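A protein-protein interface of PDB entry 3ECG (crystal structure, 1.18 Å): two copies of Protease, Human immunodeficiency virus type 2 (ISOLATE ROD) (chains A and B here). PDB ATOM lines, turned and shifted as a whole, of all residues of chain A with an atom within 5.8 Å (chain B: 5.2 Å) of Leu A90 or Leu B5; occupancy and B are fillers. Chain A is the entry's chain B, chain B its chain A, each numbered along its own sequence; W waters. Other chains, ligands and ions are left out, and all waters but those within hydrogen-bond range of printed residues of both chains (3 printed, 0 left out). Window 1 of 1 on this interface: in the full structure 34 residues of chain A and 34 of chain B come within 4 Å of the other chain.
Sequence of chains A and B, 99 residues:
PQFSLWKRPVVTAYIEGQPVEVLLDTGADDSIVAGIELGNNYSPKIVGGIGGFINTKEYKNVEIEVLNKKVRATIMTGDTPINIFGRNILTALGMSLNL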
ATOM      1  N   LEU A  24       3.043 -18.798  -7.479  1.00  0.00           N
ATOM      2  CA  LEU A  24       1.956 -19.411  -6.748  1.00  0.00           C
ATOM      3  C   LEU A  24       2.095 -20.918  -6.884  1.00  0.00           C
ATOM      4  O   LEU A  24       1.951 -21.471  -7.993  1.00  0.00           O
ATOM      5  CB  LEU A  24       0.649 -18.893  -7.334  1.00  0.00           C
ATOM      6  CG  LEU A  24       0.471 -17.350  -7.350  1.00  0.00           C
ATOM      7  CD1 LEU A  24      -0.885 -16.962  -7.925  1.00  0.00           C
ATOM      8  CD2 LEU A  24       0.665 -16.764  -5.969  1.00  0.00           C
ATOM      9  N   ASP A  25       2.360 -21.602  -5.774  1.00  0.00           N
ATOM     10  CA  ASP A  25       2.910 -22.945  -5.787  1.00  0.00           C
ATOM     11  C   ASP A  25       2.079 -23.908  -4.945  1.00  0.00           C
ATOM     12  O   ASP A  25       2.211 -24.006  -3.732  1.00  0.00           O
ATOM     13  CB  ASP A  25       4.333 -22.852  -5.206  1.00  0.00           C
ATOM     14  CG  ASP A  25       5.167 -24.078  -5.380  1.00  0.00           C
ATOM     15  OD1 ASP A  25       4.518 -25.084  -5.763  1.00  0.00           O
ATOM     16  OD2 ASP A  25       6.398 -24.034  -5.115  1.00  0.00           O
ATOM     17  N   THR A  26       1.189 -24.657  -5.592  1.00  0.00           N
ATOM     18  CA  THR A  26       0.327 -25.617  -4.915  1.00  0.00           C
ATOM     19  C   THR A  26       1.125 -26.815  -4.353  1.00  0.00           C
ATOM     20  O   THR A  26       0.578 -27.486  -3.503  1.00  0.00           O
ATOM     21  CB  THR A  26      -0.791 -26.133  -5.814  1.00  0.00           C
ATOM     22  OG1 THR A  26      -0.215 -26.773  -6.973  1.00  0.00           O
ATOM     23  CG2 THR A  26      -1.697 -25.011  -6.286  1.00  0.00           C
ATOM     24  N   PHE A  85       4.843 -18.636  -2.966  1.00  0.00           N
ATOM     25  CA  PHE A  85       3.697 -18.534  -2.090  1.00  0.00           C
ATOM     26  C   PHE A  85       3.012 -19.892  -2.136  1.00  0.00           C
ATOM     27  O   PHE A  85       2.458 -20.289  -3.161  1.00  0.00           O
ATOM     28  CB  PHE A  85       2.741 -17.423  -2.471  1.00  0.00           C
ATOM     29  CG  PHE A  85       3.136 -16.040  -2.013  1.00  0.00           C
ATOM     30  CD1 PHE A  85       2.316 -14.962  -2.333  1.00  0.00           C
ATOM     31  CD2 PHE A  85       4.295 -15.747  -1.314  1.00  0.00           C
ATOM     32  CE1 PHE A  85       2.608 -13.663  -1.968  1.00  0.00           C
ATOM     33  CE2 PHE A  85       4.593 -14.484  -0.902  1.00  0.00           C
ATOM     34  CZ  PHE A  85       3.744 -13.455  -1.224  1.00  0.00           C
ATOM     35  N   GLY A  86       3.125 -20.595  -1.026  1.00  0.00           N
ATOM     36  CA  GLY A  86       2.577 -21.935  -0.872  1.00  0.00           C
ATOM     37  C   GLY A  86       1.199 -21.894  -0.272  1.00  0.00           C
ATOM     38  O   GLY A  86       0.544 -20.868  -0.194  1.00  0.00           O
ATOM     39  N   ARG A  87       0.712 -23.060   0.097  1.00  0.00           N
ATOM     40  CA  ARG A  87      -0.691 -23.213   0.410  1.00  0.00           C
ATOM     41  C   ARG A  87      -1.128 -22.405   1.635  1.00  0.00           C
ATOM     42  O   ARG A  87      -2.314 -22.084   1.751  1.00  0.00           O
ATOM     43  CB  ARG A  87      -1.049 -24.691   0.593  1.00  0.00           C
ATOM     44  CG  ARG A  87      -0.932 -25.518  -0.672  1.00  0.00           C
ATOM     45  CD  ARG A  87      -1.376 -26.963  -0.569  1.00  0.00           C
ATOM     46  NE  ARG A  87      -0.596 -27.654   0.449  1.00  0.00           N
ATOM     47  CZ  ARG A  87      -0.931 -27.869   1.713  1.00  0.00           C
ATOM     48  NH1 ARG A  87      -2.105 -27.482   2.219  1.00  0.00           N
ATOM     49  NH2 ARG A  87      -0.058 -28.497   2.503  1.00  0.00           N
ATOM     50  N   ASN A  88      -0.232 -22.106   2.561  1.00  0.00           N
ATOM     51  CA  ASN A  88      -0.631 -21.242   3.686  1.00  0.00           C
ATOM     52  C   ASN A  88      -1.206 -19.904   3.211  1.00  0.00           C
ATOM     53  O   ASN A  88      -2.166 -19.394   3.754  1.00  0.00           O
ATOM     54  CB  ASN A  88       0.505 -21.086   4.700  1.00  0.00           C
ATOM     55  CG  ASN A  88       1.624 -20.235   4.206  1.00  0.00           C
ATOM     56  OD1 ASN A  88       2.191 -20.523   3.135  1.00  0.00           O
ATOM     57  ND2 ASN A  88       1.952 -19.201   4.964  1.00  0.00           N
ATOM     58  N   ILE A  89      -0.582 -19.355   2.163  1.00  0.00           N
ATOM     59  CA  ILE A  89      -1.096 -18.107   1.592  1.00  0.00           C
ATOM     60  C   ILE A  89      -2.188 -18.374   0.564  1.00  0.00           C
ATOM     61  O   ILE A  89      -3.167 -17.623   0.524  1.00  0.00           O
ATOM     62  CB  ILE A  89       0.060 -17.274   0.988  1.00  0.00           C
ATOM     63  CG1 ILE A  89       0.921 -16.691   2.104  1.00  0.00           C
ATOM     64  CG2 ILE A  89      -0.449 -16.210   0.023  1.00  0.00           C
ATOM     65  CD1 ILE A  89       2.192 -16.012   1.636  1.00  0.00           C
ATOM     66  N   LEU A  90      -2.054 -19.433  -0.260  1.00  0.00           N
ATOM     67  CA  LEU A  90      -3.097 -19.665  -1.255  1.00  0.00           C
ATOM     68  C   LEU A  90      -4.447 -19.862  -0.564  1.00  0.00           C
ATOM     69  O   LEU A  90      -5.462 -19.383  -1.060  1.00  0.00           O
ATOM     70  CB  LEU A  90      -2.735 -20.832  -2.184  1.00  0.00           C
ATOM     71  CG  LEU A  90      -1.386 -20.744  -2.905  1.00  0.00           C
ATOM     72  CD1 LEU A  90      -1.222 -21.910  -3.844  1.00  0.00           C
ATOM     73  CD2 LEU A  90      -1.210 -19.461  -3.713  1.00  0.00           C
ATOM     74  N   THR A  91      -4.517 -20.578   0.541  1.00  0.00           N
ATOM     75  CA  THR A  91      -5.764 -20.718   1.276  1.00  0.00           C
ATOM     76  C   THR A  91      -6.229 -19.390   1.891  1.00  0.00           C
ATOM     77  O   THR A  91      -7.424 -19.117   1.964  1.00  0.00           O
ATOM     78  CB  THR A  91      -5.681 -21.750   2.423  1.00  0.00           C
ATOM     79  OG1 THR A  91      -4.608 -21.501   3.303  1.00  0.00           O
ATOM     80  CG2 THR A  91      -5.447 -23.160   1.876  1.00  0.00           C
ATOM     81  N   ALA A  92      -5.321 -18.583   2.381  1.00  0.00           N
ATOM     82  CA  ALA A  92      -5.715 -17.312   2.944  1.00  0.00           C
ATOM     83  C   ALA A  92      -6.363 -16.444   1.881  1.00  0.00           C
ATOM     84  O   ALA A  92      -7.228 -15.660   2.157  1.00  0.00           O
ATOM     85  CB  ALA A  92      -4.494 -16.667   3.586  1.00  0.00           C
ATOM     86  N   LEU A  93      -5.954 -16.542   0.623  1.00  0.00           N
ATOM     87  CA  LEU A  93      -6.467 -15.821  -0.511  1.00  0.00           C
ATOM     88  C   LEU A  93      -7.753 -16.445  -1.051  1.00  0.00           C
ATOM     89  O   LEU A  93      -8.521 -15.835  -1.769  1.00  0.00           O
ATOM     90  CB  LEU A  93      -5.454 -15.783  -1.641  1.00  0.00           C
ATOM     91  CG  LEU A  93      -4.154 -15.035  -1.367  1.00  0.00           C
ATOM     92  CD1 LEU A  93      -3.122 -15.308  -2.449  1.00  0.00           C
ATOM     93  CD2 LEU A  93      -4.406 -13.542  -1.272  1.00  0.00           C
ATOM     94  N   GLY A  94      -8.030 -17.682  -0.678  1.00  0.00           N
ATOM     95  CA  GLY A  94      -9.220 -18.340  -1.202  1.00  0.00           C
ATOM     96  C   GLY A  94      -9.021 -19.053  -2.522  1.00  0.00           C
ATOM     97  O   GLY A  94      -9.985 -19.233  -3.271  1.00  0.00           O
ATOM     98  N   MET A  95      -7.795 -19.500  -2.829  1.00  0.00           N
ATOM     99  CA  MET A  95      -7.506 -20.032  -4.141  1.00  0.00           C
ATOM    100  C   MET A  95      -7.809 -21.521  -4.206  1.00  0.00           C
ATOM    101  O   MET A  95      -7.874 -22.207  -3.193  1.00  0.00           O
ATOM    102  CB  MET A  95      -6.036 -19.808  -4.553  1.00  0.00           C
ATOM    103  CG  MET A  95      -5.743 -18.313  -4.685  1.00  0.00           C
ATOM    104  SD  MET A  95      -4.182 -18.006  -5.519  1.00  0.00           S
ATOM    105  CE  MET A  95      -4.568 -18.236  -7.211  1.00  0.00           C
ATOM    106  N   SER A  96      -8.020 -21.991  -5.427  1.00  0.00           N
ATOM    107  CA  SER A  96      -8.339 -23.380  -5.695  1.00  0.00           C
ATOM    108  C   SER A  96      -7.690 -23.815  -7.012  1.00  0.00           C
ATOM    109  O   SER A  96      -7.422 -23.023  -7.897  1.00  0.00           O
ATOM    110  CB  SER A  96      -9.835 -23.645  -5.825  1.00  0.00           C
ATOM    111  OG  SER A  96     -10.448 -22.947  -6.856  1.00  0.00           O
ATOM    112  N   LEU A  97      -7.465 -25.102  -7.128  1.00  0.00           N
ATOM    113  CA  LEU A  97      -7.020 -25.786  -8.331  1.00  0.00           C
ATOM    114  C   LEU A  97      -8.225 -26.550  -8.879  1.00  0.00           C
ATOM    115  O   LEU A  97      -8.919 -27.250  -8.149  1.00  0.00           O
ATOM    116  CB  LEU A  97      -5.829 -26.684  -8.025  1.00  0.00           C
ATOM    117  CG  LEU A  97      -4.958 -27.333  -9.037  1.00  0.00           C
ATOM    118  CD1 LEU A  97      -4.216 -26.341  -9.893  1.00  0.00           C
ATOM    119  CD2 LEU A  97      -3.945 -28.239  -8.327  1.00  0.00           C
ATOM    120  N   PHE B   3      -9.623 -28.828  -5.990  1.00  0.00           N
ATOM    121  CA  PHE B   3      -8.682 -28.988  -4.886  1.00  0.00           C
ATOM    122  C   PHE B   3      -8.651 -27.682  -4.102  1.00  0.00           C
ATOM    123  O   PHE B   3      -8.242 -26.629  -4.614  1.00  0.00           O
ATOM    124  CB  PHE B   3      -7.302 -29.371  -5.380  1.00  0.00           C
ATOM    125  CG  PHE B   3      -7.352 -30.668  -6.169  1.00  0.00           C
ATOM    126  CD1 PHE B   3      -7.672 -30.739  -7.517  1.00  0.00           C
ATOM    127  CD2 PHE B   3      -7.107 -31.854  -5.522  1.00  0.00           C
ATOM    128  CE1 PHE B   3      -7.745 -31.981  -8.136  1.00  0.00           C
ATOM    129  CE2 PHE B   3      -7.145 -33.107  -6.109  1.00  0.00           C
ATOM    130  CZ  PHE B   3      -7.513 -33.158  -7.434  1.00  0.00           C
ATOM    131  N   SER B   4      -9.054 -27.727  -2.832  1.00  0.00           N
ATOM    132  CA  SER B   4      -9.208 -26.493  -2.064  1.00  0.00           C
ATOM    133  C   SER B   4      -7.907 -25.990  -1.418  1.00  0.00           C
ATOM    134  O   SER B   4      -7.886 -24.930  -0.837  1.00  0.00           O
ATOM    135  CB  SER B   4     -10.232 -26.696  -0.945  1.00  0.00           C
ATOM    136  OG  SER B   4      -9.653 -27.582   0.037  1.00  0.00           O
ATOM    137  N   LEU B   5      -6.853 -26.768  -1.460  1.00  0.00           N
ATOM    138  CA  LEU B   5      -5.486 -26.453  -1.061  1.00  0.00           C
ATOM    139  C   LEU B   5      -5.317 -26.372   0.445  1.00  0.00           C
ATOM    140  O   LEU B   5      -4.245 -26.055   0.901  1.00  0.00           O
ATOM    141  CB  LEU B   5      -5.031 -25.187  -1.770  1.00  0.00           C
ATOM    142  CG  LEU B   5      -5.102 -25.218  -3.297  1.00  0.00           C
ATOM    143  CD1 LEU B   5      -4.637 -23.878  -3.851  1.00  0.00           C
ATOM    144  CD2 LEU B   5      -4.287 -26.357  -3.905  1.00  0.00           C
ATOM    145  N   TRP B   6      -6.343 -26.732   1.230  1.00  0.00           N
ATOM    146  CA  TRP B   6      -6.184 -26.843   2.679  1.00  0.00           C
ATOM    147  C   TRP B   6      -5.277 -28.004   3.067  1.00  0.00           C
ATOM    148  O   TRP B   6      -4.538 -28.068   4.036  1.00  0.00           O
ATOM    149  CB  TRP B   6      -7.552 -27.013   3.369  1.00  0.00           C
ATOM    150  CG  TRP B   6      -8.329 -25.738   3.256  1.00  0.00           C
ATOM    151  CD1 TRP B   6      -9.337 -25.417   2.398  1.00  0.00           C
ATOM    152  CD2 TRP B   6      -8.097 -24.598   4.086  1.00  0.00           C
ATOM    153  NE1 TRP B   6      -9.762 -24.139   2.637  1.00  0.00           N
ATOM    154  CE2 TRP B   6      -9.018 -23.609   3.666  1.00  0.00           C
ATOM    155  CE3 TRP B   6      -7.191 -24.353   5.123  1.00  0.00           C
ATOM    156  CZ2 TRP B   6      -9.080 -22.355   4.262  1.00  0.00           C
ATOM    157  CZ3 TRP B   6      -7.272 -23.099   5.696  1.00  0.00           C
ATOM    158  CH2 TRP B   6      -8.188 -22.141   5.271  1.00  0.00           C
ATOM    159  N   LYS B   7      -5.293 -28.971   2.183  1.00  0.00           N
ATOM    160  CA  LYS B   7      -4.415 -30.119   2.201  1.00  0.00           C
ATOM    161  C   LYS B   7      -3.575 -30.224   0.928  1.00  0.00           C
ATOM    162  O   LYS B   7      -3.916 -29.595  -0.098  1.00  0.00           O
ATOM    163  CB  LYS B   7      -5.223 -31.420   2.452  1.00  0.00           C
ATOM    164  CG  LYS B   7      -6.430 -31.621   1.587  1.00  0.00           C
ATOM    165  CD  LYS B   7      -7.472 -32.537   2.178  1.00  0.00           C
ATOM    166  CE  LYS B   7      -7.038 -33.969   2.364  1.00  0.00           C
ATOM    167  NZ  LYS B   7      -6.907 -34.703   1.076  1.00  0.00           N
ATOM    168  N   PRO B   9      -2.559 -31.312  -2.607  1.00  0.00           N
ATOM    169  CA  PRO B   9      -3.321 -31.927  -3.686  1.00  0.00           C
ATOM    170  C   PRO B   9      -2.617 -33.157  -4.279  1.00  0.00           C
ATOM    171  O   PRO B   9      -1.864 -33.071  -5.227  1.00  0.00           O
ATOM    172  CB  PRO B   9      -3.473 -30.813  -4.686  1.00  0.00           C
ATOM    173  CG  PRO B   9      -2.213 -30.009  -4.491  1.00  0.00           C
ATOM    174  CD  PRO B   9      -1.977 -30.024  -3.023  1.00  0.00           C
ATOM    175  N   LEU B  97      -5.567 -22.674 -11.970  1.00  0.00           N
ATOM    176  CA  LEU B  97      -5.461 -22.140 -10.619  1.00  0.00           C
ATOM    177  C   LEU B  97      -6.307 -20.869 -10.559  1.00  0.00           C
ATOM    178  O   LEU B  97      -6.094 -19.967 -11.366  1.00  0.00           O
ATOM    179  CB  LEU B  97      -3.981 -21.945 -10.312  1.00  0.00           C
ATOM    180  CG  LEU B  97      -3.621 -21.355  -8.978  1.00  0.00           C
ATOM    181  CD1 LEU B  97      -3.945 -22.345  -7.872  1.00  0.00           C
ATOM    182  CD2 LEU B  97      -2.148 -20.991  -9.016  1.00  0.00           C
HETATM  183  O   HOH W   1      -8.401 -22.295  -0.661  1.00  0.00           O
HETATM  184  O   HOH W   2      -1.880 -28.564   5.153  1.00  0.00           O
HETATM  185  O   HOH W   3      -9.632 -21.007   1.117  1.00  0.00           O
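The backbone NH of Phe B3 lies within hydrogen-bond range of the backbone carbonyl oxygen of Leu A97, at 2.8 Å.
O of Leu B5 lies within hydrogen-bond range of NH1 of Arg A87.
NH1 of Arg A87 is in hydrogen-bond range of O of Trp B6 (3.1 Å).
O of Leu A90 sits at hydrogen-bond distance from N of Met A95, at 2.9 Å.
The backbone carbonyl oxygen (O) of Asn A88 lies within hydrogen-bond range of the side-chain hydroxyl (OG1) of Thr A91 (3.3 Å).
The backbone carbonyl oxygen (O) of Arg A87 lies within hydrogen-bond range of the side-chain hydroxyl (OG1) of Thr A91 (2.8 Å).
Among the printed residues, pairs that only touch across the chains: Thr A91 with Leu B5 (3.3 Å), Arg A87 with Lys B7 (3.4 Å), Ser A96 with Phe B3 (3.4 Å), Ser A96 with Leu B97 (3.5 Å), Met A95 with Ser B4 (3.6 Å), Thr A26 with Pro B9 (3.6 Å), Met A95 with Leu B5 (3.7 Å), Met A95 with Leu B97 (3.7 Å), Thr A91 with Trp B6 (3.7 Å), Thr A26 with Leu B5 (3.8 Å), Thr A26 with Leu B97 (3.8 Å), Leu A24 with Leu B97 (3.9 Å), Leu A90 with Leu B5 (3.9 Å) and Arg A87 with Pro B9 (3.97 Å).
Of the printed residues of chain B, Thr A26 touches Leu B5, Pro B9 and Leu B97.
Of the printed residues of chain B, Thr A91 touches Leu B5 and Trp B6.
Of the printed residues of chain B, Ser A96 touches Phe B3 (3.4 Å) and Leu B97 (3.5 Å).
Printed residues of chain A within 4 Å of Ser B4: Met A95.
Of the printed residues of chain A, Leu B5 touches Thr A26 (3.8 Å), Arg A87 (2.9 Å), Leu A90 (3.9 Å), Thr A91 (3.3 Å) and Met A95 (3.7 Å).
The nearest residue of chain B that does not touch Leu A90 is Leu B97 (4.9 Å).
The nearest residue of chain A that does not touch Leu B5 is Ser A96 (4.2 Å).
The nearest printed residue of chain A that does not touch Pro B9 is Leu A97 (4.5 Å).
Hydrophobic or aromatic side chains of chain A that line the printed part of chain B: Leu A24, Leu A90 and Met A95.
Of the 7 printed residues of chain B, 7 touch a printed residue of chain A.
Along chain B the printed residues that touch a printed residue of chain A span positions 3 to 97.
Among the printed residues, no Asp or Glu carboxylate lies within 4 Å of a Lys or Arg side-chain nitrogen of the other chain.
Position printed for both chains: 97.
Of the 17 pairs that touch across the chains among the printed residues, none has its exchanged pair printed and touching as well.
Water W1 bridges the backbone carbonyl oxygen of Met A95 (2.6 Å) and the backbone carbonyl oxygen of Ser B4 (2.7 Å).
Water W2 bridges O of Trp B6 (2.9 Å) and NH1 of Arg A87 (3.1 Å).
Water W3 bridges the backbone carbonyl oxygen (O) of Thr A91 (3.0 Å) and the indole nitrogen (NE1) of Trp B6 (3.5 Å).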
